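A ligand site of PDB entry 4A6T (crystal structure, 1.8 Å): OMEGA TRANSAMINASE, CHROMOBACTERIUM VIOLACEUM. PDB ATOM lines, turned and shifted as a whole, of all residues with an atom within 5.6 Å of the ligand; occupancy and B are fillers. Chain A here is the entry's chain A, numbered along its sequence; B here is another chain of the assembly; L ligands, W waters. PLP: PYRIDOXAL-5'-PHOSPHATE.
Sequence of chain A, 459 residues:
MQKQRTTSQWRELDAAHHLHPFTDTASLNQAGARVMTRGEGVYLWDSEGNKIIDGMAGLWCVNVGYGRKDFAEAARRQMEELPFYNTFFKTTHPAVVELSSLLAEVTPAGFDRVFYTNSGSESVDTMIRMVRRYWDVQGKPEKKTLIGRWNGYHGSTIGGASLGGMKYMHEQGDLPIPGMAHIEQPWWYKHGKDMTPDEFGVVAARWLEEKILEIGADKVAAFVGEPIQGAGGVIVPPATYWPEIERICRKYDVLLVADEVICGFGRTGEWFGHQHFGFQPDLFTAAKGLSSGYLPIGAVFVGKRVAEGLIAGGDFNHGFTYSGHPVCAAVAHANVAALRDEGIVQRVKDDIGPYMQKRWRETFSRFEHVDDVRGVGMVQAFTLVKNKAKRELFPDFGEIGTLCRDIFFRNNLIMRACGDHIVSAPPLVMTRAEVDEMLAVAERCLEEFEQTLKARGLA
The side-chain hydroxyl of Ser 121 sits at hydrogen-bond distance from the backbone NH of Ser 156.
OG of Ser 119 sits at hydrogen-bond distance from N of Glu 122 of chain A.
The side-chain carboxylate of Asp 259 lies close to the backbone NH of Val 261 (3.1 Å).
N of Ser 121 sits close to OG of Ser 119.
The backbone NH (N) of Tyr 153 lies within hydrogen-bond range of the side-chain carboxylate (OE2) of Glu 226 (2.9 Å).
The side-chain hydroxyl (OH) of Tyr 322 of chain B lies within hydrogen-bond range of the backbone carbonyl oxygen (O) of Lys 288 (2.9 Å).
OE2 of Glu 122 of chain B lies within hydrogen-bond range of OG of Ser 119, at 2.5 Å.
CB of Ser 119 touches O2P of the ligand, at 3.5 Å.
Tyr 153 touches the ligand.
His 154 touches the ligand (C to C6, 3.6 Å).
Gly 155 touches the ligand (N to C6, 3.5 Å).
Glu 226 touches the ligand (OE1 to C2A, 3.4 Å).
Val 261 touches the ligand (CG1 to C4, 3.4 Å).
CG1 of Ile 262 touches O3 of the ligand, at 3.1 Å.
Phe 320 of chain B touches the ligand.
Of the 25 residues printed, 13 come within 4 Å of the ligand.
Along chain A the residues within 4 Å of the ligand span positions 119 to 288.
Water W4 lies within hydrogen-bond range of an oxygen (O2P) of the ligand and the backbone NH (N) of Lys 288.
Water W3 lies within hydrogen-bond range of O1P of the ligand, OH of Tyr 153 and O of Gly 319 of chain B.
Water W2 lies within hydrogen-bond range of OE1 of Glu 226, N of Ala 231 and O3 of the ligand.
An oxygen (O3P) of the ligand lies within hydrogen-bond range of the side-chain hydroxyl (OG) of Ser 121 (2.5 Å).
N of Thr 321 of chain B is in hydrogen-bond range of O1P of the ligand, 2.9 Å away.
O1P of the ligand sits at hydrogen-bond distance from OG1 of Thr 321 of chain B, at 2.7 Å.
N1 of the ligand is in hydrogen-bond range of OD2 of Asp 259.
The backbone NH (N) of Gly 120 lies within hydrogen-bond range of an oxygen (O2P) of the ligand (3.0 Å).
NZ of Lys 288 is covalently linked to C4A of the ligand.
N of Ser 121 is in hydrogen-bond range of O3P of the ligand, 2.7 Å away.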
ATOM      1  N   TRP A  60       7.693  20.190  14.873  1.00  0.00           N
ATOM      2  CA  TRP A  60       7.112  21.499  15.200  1.00  0.00           C
ATOM      3  C   TRP A  60       7.803  22.644  14.462  1.00  0.00           C
ATOM      4  O   TRP A  60       7.727  23.788  14.931  1.00  0.00           O
ATOM      5  CB  TRP A  60       7.226  21.828  16.695  1.00  0.00           C
ATOM      6  CG  TRP A  60       6.957  20.742  17.717  1.00  0.00           C
ATOM      7  CD1 TRP A  60       7.823  19.759  18.108  1.00  0.00           C
ATOM      8  CD2 TRP A  60       5.778  20.584  18.514  1.00  0.00           C
ATOM      9  NE1 TRP A  60       7.245  18.989  19.087  1.00  0.00           N
ATOM     10  CE2 TRP A  60       5.996  19.468  19.353  1.00  0.00           C
ATOM     11  CE3 TRP A  60       4.567  21.255  18.595  1.00  0.00           C
ATOM     12  CZ2 TRP A  60       5.028  19.021  20.259  1.00  0.00           C
ATOM     13  CZ3 TRP A  60       3.611  20.807  19.494  1.00  0.00           C
ATOM     14  CH2 TRP A  60       3.850  19.700  20.312  1.00  0.00           C
ATOM     15  N   ASN A 118      23.141  27.345  17.349  1.00  0.00           N
ATOM     16  CA  ASN A 118      22.858  26.311  16.357  1.00  0.00           C
ATOM     17  C   ASN A 118      21.555  25.581  16.625  1.00  0.00           C
ATOM     18  O   ASN A 118      21.056  24.873  15.748  1.00  0.00           O
ATOM     19  CB  ASN A 118      24.001  25.295  16.339  1.00  0.00           C
ATOM     20  CG  ASN A 118      25.323  25.925  15.988  1.00  0.00           C
ATOM     21  OD1 ASN A 118      25.499  26.434  14.885  1.00  0.00           O
ATOM     22  ND2 ASN A 118      26.259  25.907  16.924  1.00  0.00           N
ATOM     23  N   SER A 119      21.006  25.750  17.824  1.00  0.00           N
ATOM     24  CA  SER A 119      19.844  24.993  18.254  1.00  0.00           C
ATOM     25  C   SER A 119      19.074  25.718  19.343  1.00  0.00           C
ATOM     26  O   SER A 119      19.570  26.671  19.950  1.00  0.00           O
ATOM     27  CB  SER A 119      20.290  23.646  18.806  1.00  0.00           C
ATOM     28  OG  SER A 119      20.983  23.826  20.038  1.00  0.00           O
ATOM     29  N   GLY A 120      17.855  25.262  19.604  1.00  0.00           N
ATOM     30  CA  GLY A 120      17.080  25.770  20.718  1.00  0.00           C
ATOM     31  C   GLY A 120      17.718  25.444  22.062  1.00  0.00           C
ATOM     32  O   GLY A 120      17.629  26.234  23.001  1.00  0.00           O
ATOM     33  N   SER A 121      18.361  24.284  22.157  1.00  0.00           N
ATOM     34  CA  SER A 121      19.031  23.873  23.395  1.00  0.00           C
ATOM     35  C   SER A 121      20.178  24.834  23.728  1.00  0.00           C
ATOM     36  O   SER A 121      20.357  25.208  24.887  1.00  0.00           O
ATOM     37  CB  SER A 121      19.552  22.444  23.275  1.00  0.00           C
ATOM     38  OG  SER A 121      18.500  21.510  23.233  1.00  0.00           O
ATOM     39  N   GLU A 122      20.954  25.218  22.730  1.00  0.00           N
ATOM     40  CA  GLU A 122      22.058  26.140  22.931  1.00  0.00           C
ATOM     41  C   GLU A 122      21.526  27.528  23.246  1.00  0.00           C
ATOM     42  O   GLU A 122      22.127  28.276  24.022  1.00  0.00           O
ATOM     43  CB  GLU A 122      22.933  26.208  21.671  1.00  0.00           C
ATOM     44  CG  GLU A 122      23.764  24.969  21.408  1.00  0.00           C
ATOM     45  CD  GLU A 122      24.515  25.066  20.093  1.00  0.00           C
ATOM     46  OE1 GLU A 122      24.502  26.164  19.488  1.00  0.00           O
ATOM     47  OE2 GLU A 122      25.128  24.066  19.669  1.00  0.00           O
ATOM     48  N   VAL A 124      18.843  28.103  24.934  1.00  0.00           N
ATOM     49  CA  VAL A 124      18.488  28.056  26.348  1.00  0.00           C
ATOM     50  C   VAL A 124      19.724  28.180  27.252  1.00  0.00           C
ATOM     51  O   VAL A 124      19.681  28.902  28.240  1.00  0.00           O
ATOM     52  CB  VAL A 124      17.653  26.788  26.660  1.00  0.00           C
ATOM     53  CG1 VAL A 124      17.443  26.643  28.150  1.00  0.00           C
ATOM     54  CG2 VAL A 124      16.310  26.875  25.928  1.00  0.00           C
ATOM     55  N   TYR A 153       9.520  21.974  28.771  1.00  0.00           N
ATOM     56  CA  TYR A 153      10.649  21.475  27.999  1.00  0.00           C
ATOM     57  C   TYR A 153      11.470  22.649  27.467  1.00  0.00           C
ATOM     58  O   TYR A 153      10.923  23.560  26.857  1.00  0.00           O
ATOM     59  CB  TYR A 153      10.182  20.624  26.816  1.00  0.00           C
ATOM     60  CG  TYR A 153      11.352  19.972  26.115  1.00  0.00           C
ATOM     61  CD1 TYR A 153      11.988  18.873  26.666  1.00  0.00           C
ATOM     62  CD2 TYR A 153      11.833  20.472  24.908  1.00  0.00           C
ATOM     63  CE1 TYR A 153      13.067  18.278  26.043  1.00  0.00           C
ATOM     64  CE2 TYR A 153      12.925  19.875  24.264  1.00  0.00           C
ATOM     65  CZ  TYR A 153      13.540  18.785  24.849  1.00  0.00           C
ATOM     66  OH  TYR A 153      14.602  18.187  24.240  1.00  0.00           O
ATOM     67  N   HIS A 154      12.777  22.586  27.693  1.00  0.00           N
ATOM     68  CA  HIS A 154      13.656  23.672  27.312  1.00  0.00           C
ATOM     69  C   HIS A 154      14.957  23.141  26.733  1.00  0.00           C
ATOM     70  O   HIS A 154      16.015  23.764  26.865  1.00  0.00           O
ATOM     71  CB  HIS A 154      13.902  24.552  28.529  1.00  0.00           C
ATOM     72  CG  HIS A 154      12.648  25.185  29.031  1.00  0.00           C
ATOM     73  ND1 HIS A 154      12.042  24.834  30.223  1.00  0.00           N
ATOM     74  CD2 HIS A 154      11.825  26.104  28.462  1.00  0.00           C
ATOM     75  CE1 HIS A 154      10.936  25.535  30.374  1.00  0.00           C
ATOM     76  NE2 HIS A 154      10.786  26.317  29.324  1.00  0.00           N
ATOM     77  N   GLY A 155      14.863  21.985  26.097  1.00  0.00           N
ATOM     78  CA  GLY A 155      15.988  21.438  25.386  1.00  0.00           C
ATOM     79  C   GLY A 155      16.741  20.349  26.109  1.00  0.00           C
ATOM     80  O   GLY A 155      16.306  19.840  27.163  1.00  0.00           O
ATOM     81  N   SER A 156      17.889  20.001  25.560  1.00  0.00           N
ATOM     82  CA  SER A 156      18.571  18.775  25.931  1.00  0.00           C
ATOM     83  C   SER A 156      20.047  18.963  26.267  1.00  0.00           C
ATOM     84  O   SER A 156      20.783  17.995  26.412  1.00  0.00           O
ATOM     85  CB  SER A 156      18.431  17.748  24.814  1.00  0.00           C
ATOM     86  OG  SER A 156      19.023  16.538  25.195  1.00  0.00           O
ATOM     87  N   GLU A 226       7.482  28.146  28.291  1.00  0.00           N
ATOM     88  CA  GLU A 226       6.906  28.138  26.949  1.00  0.00           C
ATOM     89  C   GLU A 226       5.509  28.765  27.035  1.00  0.00           C
ATOM     90  O   GLU A 226       4.737  28.425  27.930  1.00  0.00           O
ATOM     91  CB  GLU A 226       6.731  26.712  26.447  1.00  0.00           C
ATOM     92  CG  GLU A 226       7.978  25.830  26.421  1.00  0.00           C
ATOM     93  CD  GLU A 226       7.624  24.355  26.508  1.00  0.00           C
ATOM     94  OE1 GLU A 226       7.383  23.715  25.456  1.00  0.00           O
ATOM     95  OE2 GLU A 226       7.541  23.840  27.650  1.00  0.00           O
ATOM     96  N   ALA A 231       6.201  19.883  24.137  1.00  0.00           N
ATOM     97  CA  ALA A 231       6.505  18.472  24.329  1.00  0.00           C
ATOM     98  C   ALA A 231       5.705  17.931  25.503  1.00  0.00           C
ATOM     99  O   ALA A 231       5.468  16.725  25.599  1.00  0.00           O
ATOM    100  CB  ALA A 231       8.003  18.279  24.556  1.00  0.00           C
ATOM    101  N   ASP A 259      10.233  30.940  26.298  1.00  0.00           N
ATOM    102  CA  ASP A 259      10.876  30.019  25.378  1.00  0.00           C
ATOM    103  C   ASP A 259       9.951  29.887  24.172  1.00  0.00           C
ATOM    104  O   ASP A 259       8.921  29.210  24.251  1.00  0.00           O
ATOM    105  CB  ASP A 259      11.110  28.656  26.033  1.00  0.00           C
ATOM    106  CG  ASP A 259      11.980  27.743  25.190  1.00  0.00           C
ATOM    107  OD1 ASP A 259      12.138  28.036  23.983  1.00  0.00           O
ATOM    108  OD2 ASP A 259      12.497  26.734  25.715  1.00  0.00           O
ATOM    109  N   VAL A 261      10.762  28.585  21.273  1.00  0.00           N
ATOM    110  CA  VAL A 261      11.308  27.663  20.294  1.00  0.00           C
ATOM    111  C   VAL A 261      10.193  27.012  19.460  1.00  0.00           C
ATOM    112  O   VAL A 261      10.362  26.841  18.258  1.00  0.00           O
ATOM    113  CB  VAL A 261      12.255  26.634  20.932  1.00  0.00           C
ATOM    114  CG1 VAL A 261      12.609  25.573  19.931  1.00  0.00           C
ATOM    115  CG2 VAL A 261      13.521  27.325  21.426  1.00  0.00           C
ATOM    116  N   ILE A 262       9.062  26.680  20.061  1.00  0.00           N
ATOM    117  CA  ILE A 262       7.942  26.143  19.273  1.00  0.00           C
ATOM    118  C   ILE A 262       6.947  27.212  18.808  1.00  0.00           C
ATOM    119  O   ILE A 262       6.549  27.212  17.647  1.00  0.00           O
ATOM    120  CB  ILE A 262       7.174  25.049  20.027  1.00  0.00           C
ATOM    121  CG1 ILE A 262       7.931  23.718  19.940  1.00  0.00           C
ATOM    122  CG2 ILE A 262       5.793  24.886  19.414  1.00  0.00           C
ATOM    123  CD1 ILE A 262       7.319  22.607  20.777  1.00  0.00           C
ATOM    124  N   ALA A 287      14.322  28.985  17.751  1.00  0.00           N
ATOM    125  CA  ALA A 287      14.979  28.038  16.862  1.00  0.00           C
ATOM    126  C   ALA A 287      13.856  27.471  15.985  1.00  0.00           C
ATOM    127  O   ALA A 287      12.926  28.193  15.636  1.00  0.00           O
ATOM    128  CB  ALA A 287      15.669  26.939  17.649  1.00  0.00           C
ATOM    129  N   LYS A 288      13.928  26.187  15.649  1.00  0.00           N
ATOM    130  CA  LYS A 288      12.848  25.520  14.838  1.00  0.00           C
ATOM    131  C   LYS A 288      12.393  26.405  13.686  1.00  0.00           C
ATOM    132  O   LYS A 288      13.078  26.482  12.655  1.00  0.00           O
ATOM    133  CB  LYS A 288      11.726  25.060  15.791  1.00  0.00           C
ATOM    134  CG  LYS A 288      12.215  23.850  16.610  1.00  0.00           C
ATOM    135  CD  LYS A 288      11.137  23.171  17.468  1.00  0.00           C
ATOM    136  CE  LYS A 288      11.713  21.954  18.240  1.00  0.00           C
ATOM    137  NZ  LYS A 288      11.576  22.098  19.687  1.00  0.00           N
ATOM    138  N   PHE B  88      13.641  11.170  15.729  1.00  0.00           N
ATOM    139  CA  PHE B  88      13.007  10.911  17.032  1.00  0.00           C
ATOM    140  C   PHE B  88      11.883   9.897  16.974  1.00  0.00           C
ATOM    141  O   PHE B  88      11.602   9.219  17.954  1.00  0.00           O
ATOM    142  CB  PHE B  88      12.344  12.189  17.573  1.00  0.00           C
ATOM    143  CG  PHE B  88      13.292  13.226  18.093  1.00  0.00           C
ATOM    144  CD1 PHE B  88      14.289  13.756  17.288  1.00  0.00           C
ATOM    145  CD2 PHE B  88      13.140  13.711  19.383  1.00  0.00           C
ATOM    146  CE1 PHE B  88      15.133  14.736  17.774  1.00  0.00           C
ATOM    147  CE2 PHE B  88      13.997  14.692  19.877  1.00  0.00           C
ATOM    148  CZ  PHE B  88      14.998  15.209  19.065  1.00  0.00           C
ATOM    149  N   ASN B 118      24.591  19.349  16.739  1.00  0.00           N
ATOM    150  CA  ASN B 118      24.838  20.488  15.847  1.00  0.00           C
ATOM    151  C   ASN B 118      26.145  21.204  16.099  1.00  0.00           C
ATOM    152  O   ASN B 118      26.521  22.117  15.350  1.00  0.00           O
ATOM    153  CB  ASN B 118      23.713  21.523  15.956  1.00  0.00           C
ATOM    154  CG  ASN B 118      22.350  20.910  15.793  1.00  0.00           C
ATOM    155  OD1 ASN B 118      21.990  20.456  14.700  1.00  0.00           O
ATOM    156  ND2 ASN B 118      21.573  20.898  16.866  1.00  0.00           N
ATOM    157  N   GLU B 122      27.534  20.838  21.967  1.00  0.00           N
ATOM    158  CA  GLU B 122      26.468  19.869  22.205  1.00  0.00           C
ATOM    159  C   GLU B 122      27.023  18.446  22.312  1.00  0.00           C
ATOM    160  O   GLU B 122      26.494  17.615  23.064  1.00  0.00           O
ATOM    161  CB  GLU B 122      25.416  19.930  21.106  1.00  0.00           C
ATOM    162  CG  GLU B 122      24.596  21.213  21.068  1.00  0.00           C
ATOM    163  CD  GLU B 122      23.634  21.219  19.905  1.00  0.00           C
ATOM    164  OE1 GLU B 122      23.715  20.298  19.062  1.00  0.00           O
ATOM    165  OE2 GLU B 122      22.793  22.139  19.825  1.00  0.00           O
ATOM    166  N   GLY B 319      18.901  14.518  23.163  1.00  0.00           N
ATOM    167  CA  GLY B 319      19.026  14.741  21.742  1.00  0.00           C
ATOM    168  C   GLY B 319      18.461  16.060  21.288  1.00  0.00           C
ATOM    169  O   GLY B 319      17.791  16.759  22.041  1.00  0.00           O
ATOM    170  N   PHE B 320      18.732  16.379  20.033  1.00  0.00           N
ATOM    171  CA  PHE B 320      18.390  17.682  19.501  1.00  0.00           C
ATOM    172  C   PHE B 320      17.557  17.546  18.227  1.00  0.00           C
ATOM    173  O   PHE B 320      17.716  16.605  17.459  1.00  0.00           O
ATOM    174  CB  PHE B 320      19.683  18.465  19.236  1.00  0.00           C
ATOM    175  CG  PHE B 320      20.631  18.443  20.406  1.00  0.00           C
ATOM    176  CD1 PHE B 320      20.487  19.354  21.447  1.00  0.00           C
ATOM    177  CD2 PHE B 320      21.648  17.503  20.471  1.00  0.00           C
ATOM    178  CE1 PHE B 320      21.348  19.323  22.531  1.00  0.00           C
ATOM    179  CE2 PHE B 320      22.509  17.471  21.555  1.00  0.00           C
ATOM    180  CZ  PHE B 320      22.360  18.376  22.589  1.00  0.00           C
ATOM    181  N   THR B 321      16.673  18.528  18.027  1.00  0.00           N
ATOM    182  CA  THR B 321      15.760  18.551  16.893  1.00  0.00           C
ATOM    183  C   THR B 321      16.503  18.341  15.582  1.00  0.00           C
ATOM    184  O   THR B 321      16.082  17.557  14.728  1.00  0.00           O
ATOM    185  CB  THR B 321      15.046  19.920  16.828  1.00  0.00           C
ATOM    186  OG1 THR B 321      14.256  20.104  18.012  1.00  0.00           O
ATOM    187  CG2 THR B 321      14.155  20.028  15.602  1.00  0.00           C
ATOM    188  N   TYR B 322      17.610  19.059  15.416  1.00  0.00           N
ATOM    189  CA  TYR B 322      18.401  18.971  14.189  1.00  0.00           C
ATOM    190  C   TYR B 322      19.507  17.917  14.259  1.00  0.00           C
ATOM    191  O   TYR B 322      20.402  17.896  13.411  1.00  0.00           O
ATOM    192  CB  TYR B 322      19.002  20.347  13.876  1.00  0.00           C
ATOM    193  CG  TYR B 322      17.962  21.441  13.698  1.00  0.00           C
ATOM    194  CD1 TYR B 322      16.749  21.183  13.069  1.00  0.00           C
ATOM    195  CD2 TYR B 322      18.202  22.733  14.148  1.00  0.00           C
ATOM    196  CE1 TYR B 322      15.804  22.186  12.887  1.00  0.00           C
ATOM    197  CE2 TYR B 322      17.258  23.754  13.965  1.00  0.00           C
ATOM    198  CZ  TYR B 322      16.068  23.460  13.340  1.00  0.00           C
ATOM    199  OH  TYR B 322      15.118  24.441  13.167  1.00  0.00           O
HETATM  200  N1  PLP L   1      12.677  24.639  23.910  1.00  0.00           N
HETATM  201  C2  PLP L   1      11.476  24.264  23.412  1.00  0.00           C
HETATM  202  C2A PLP L   1      10.195  24.864  23.930  1.00  0.00           C
HETATM  203  C3  PLP L   1      11.401  23.260  22.324  1.00  0.00           C
HETATM  204  O3  PLP L   1      10.204  22.872  21.820  1.00  0.00           O
HETATM  205  C4  PLP L   1      12.658  22.678  21.804  1.00  0.00           C
HETATM  206  C4A PLP L   1      12.567  21.648  20.675  1.00  0.00           C
HETATM  207  C5  PLP L   1      13.907  23.168  22.450  1.00  0.00           C
HETATM  208  C6  PLP L   1      13.839  24.126  23.474  1.00  0.00           C
HETATM  209  C5A PLP L   1      15.286  22.680  22.067  1.00  0.00           C
HETATM  210  O4P PLP L   1      15.597  22.888  20.695  1.00  0.00           O
HETATM  211  P   PLP L   1      16.711  21.948  19.981  1.00  0.00           P
HETATM  212  O1P PLP L   1      16.048  20.596  19.922  1.00  0.00           O
HETATM  213  O2P PLP L   1      16.925  22.610  18.639  1.00  0.00           O
HETATM  214  O3P PLP L   1      17.922  21.957  20.887  1.00  0.00           O
HETATM  215  O   HOH W   1      18.503  21.207  16.991  1.00  0.00           O
HETATM  216  O   HOH W   2       8.440  21.732  23.963  1.00  0.00           O
HETATM  217  O   HOH W   3      15.813  18.811  21.898  1.00  0.00           O
HETATM  218  O   HOH W   4      15.690  23.617  16.703  1.00  0.00           O
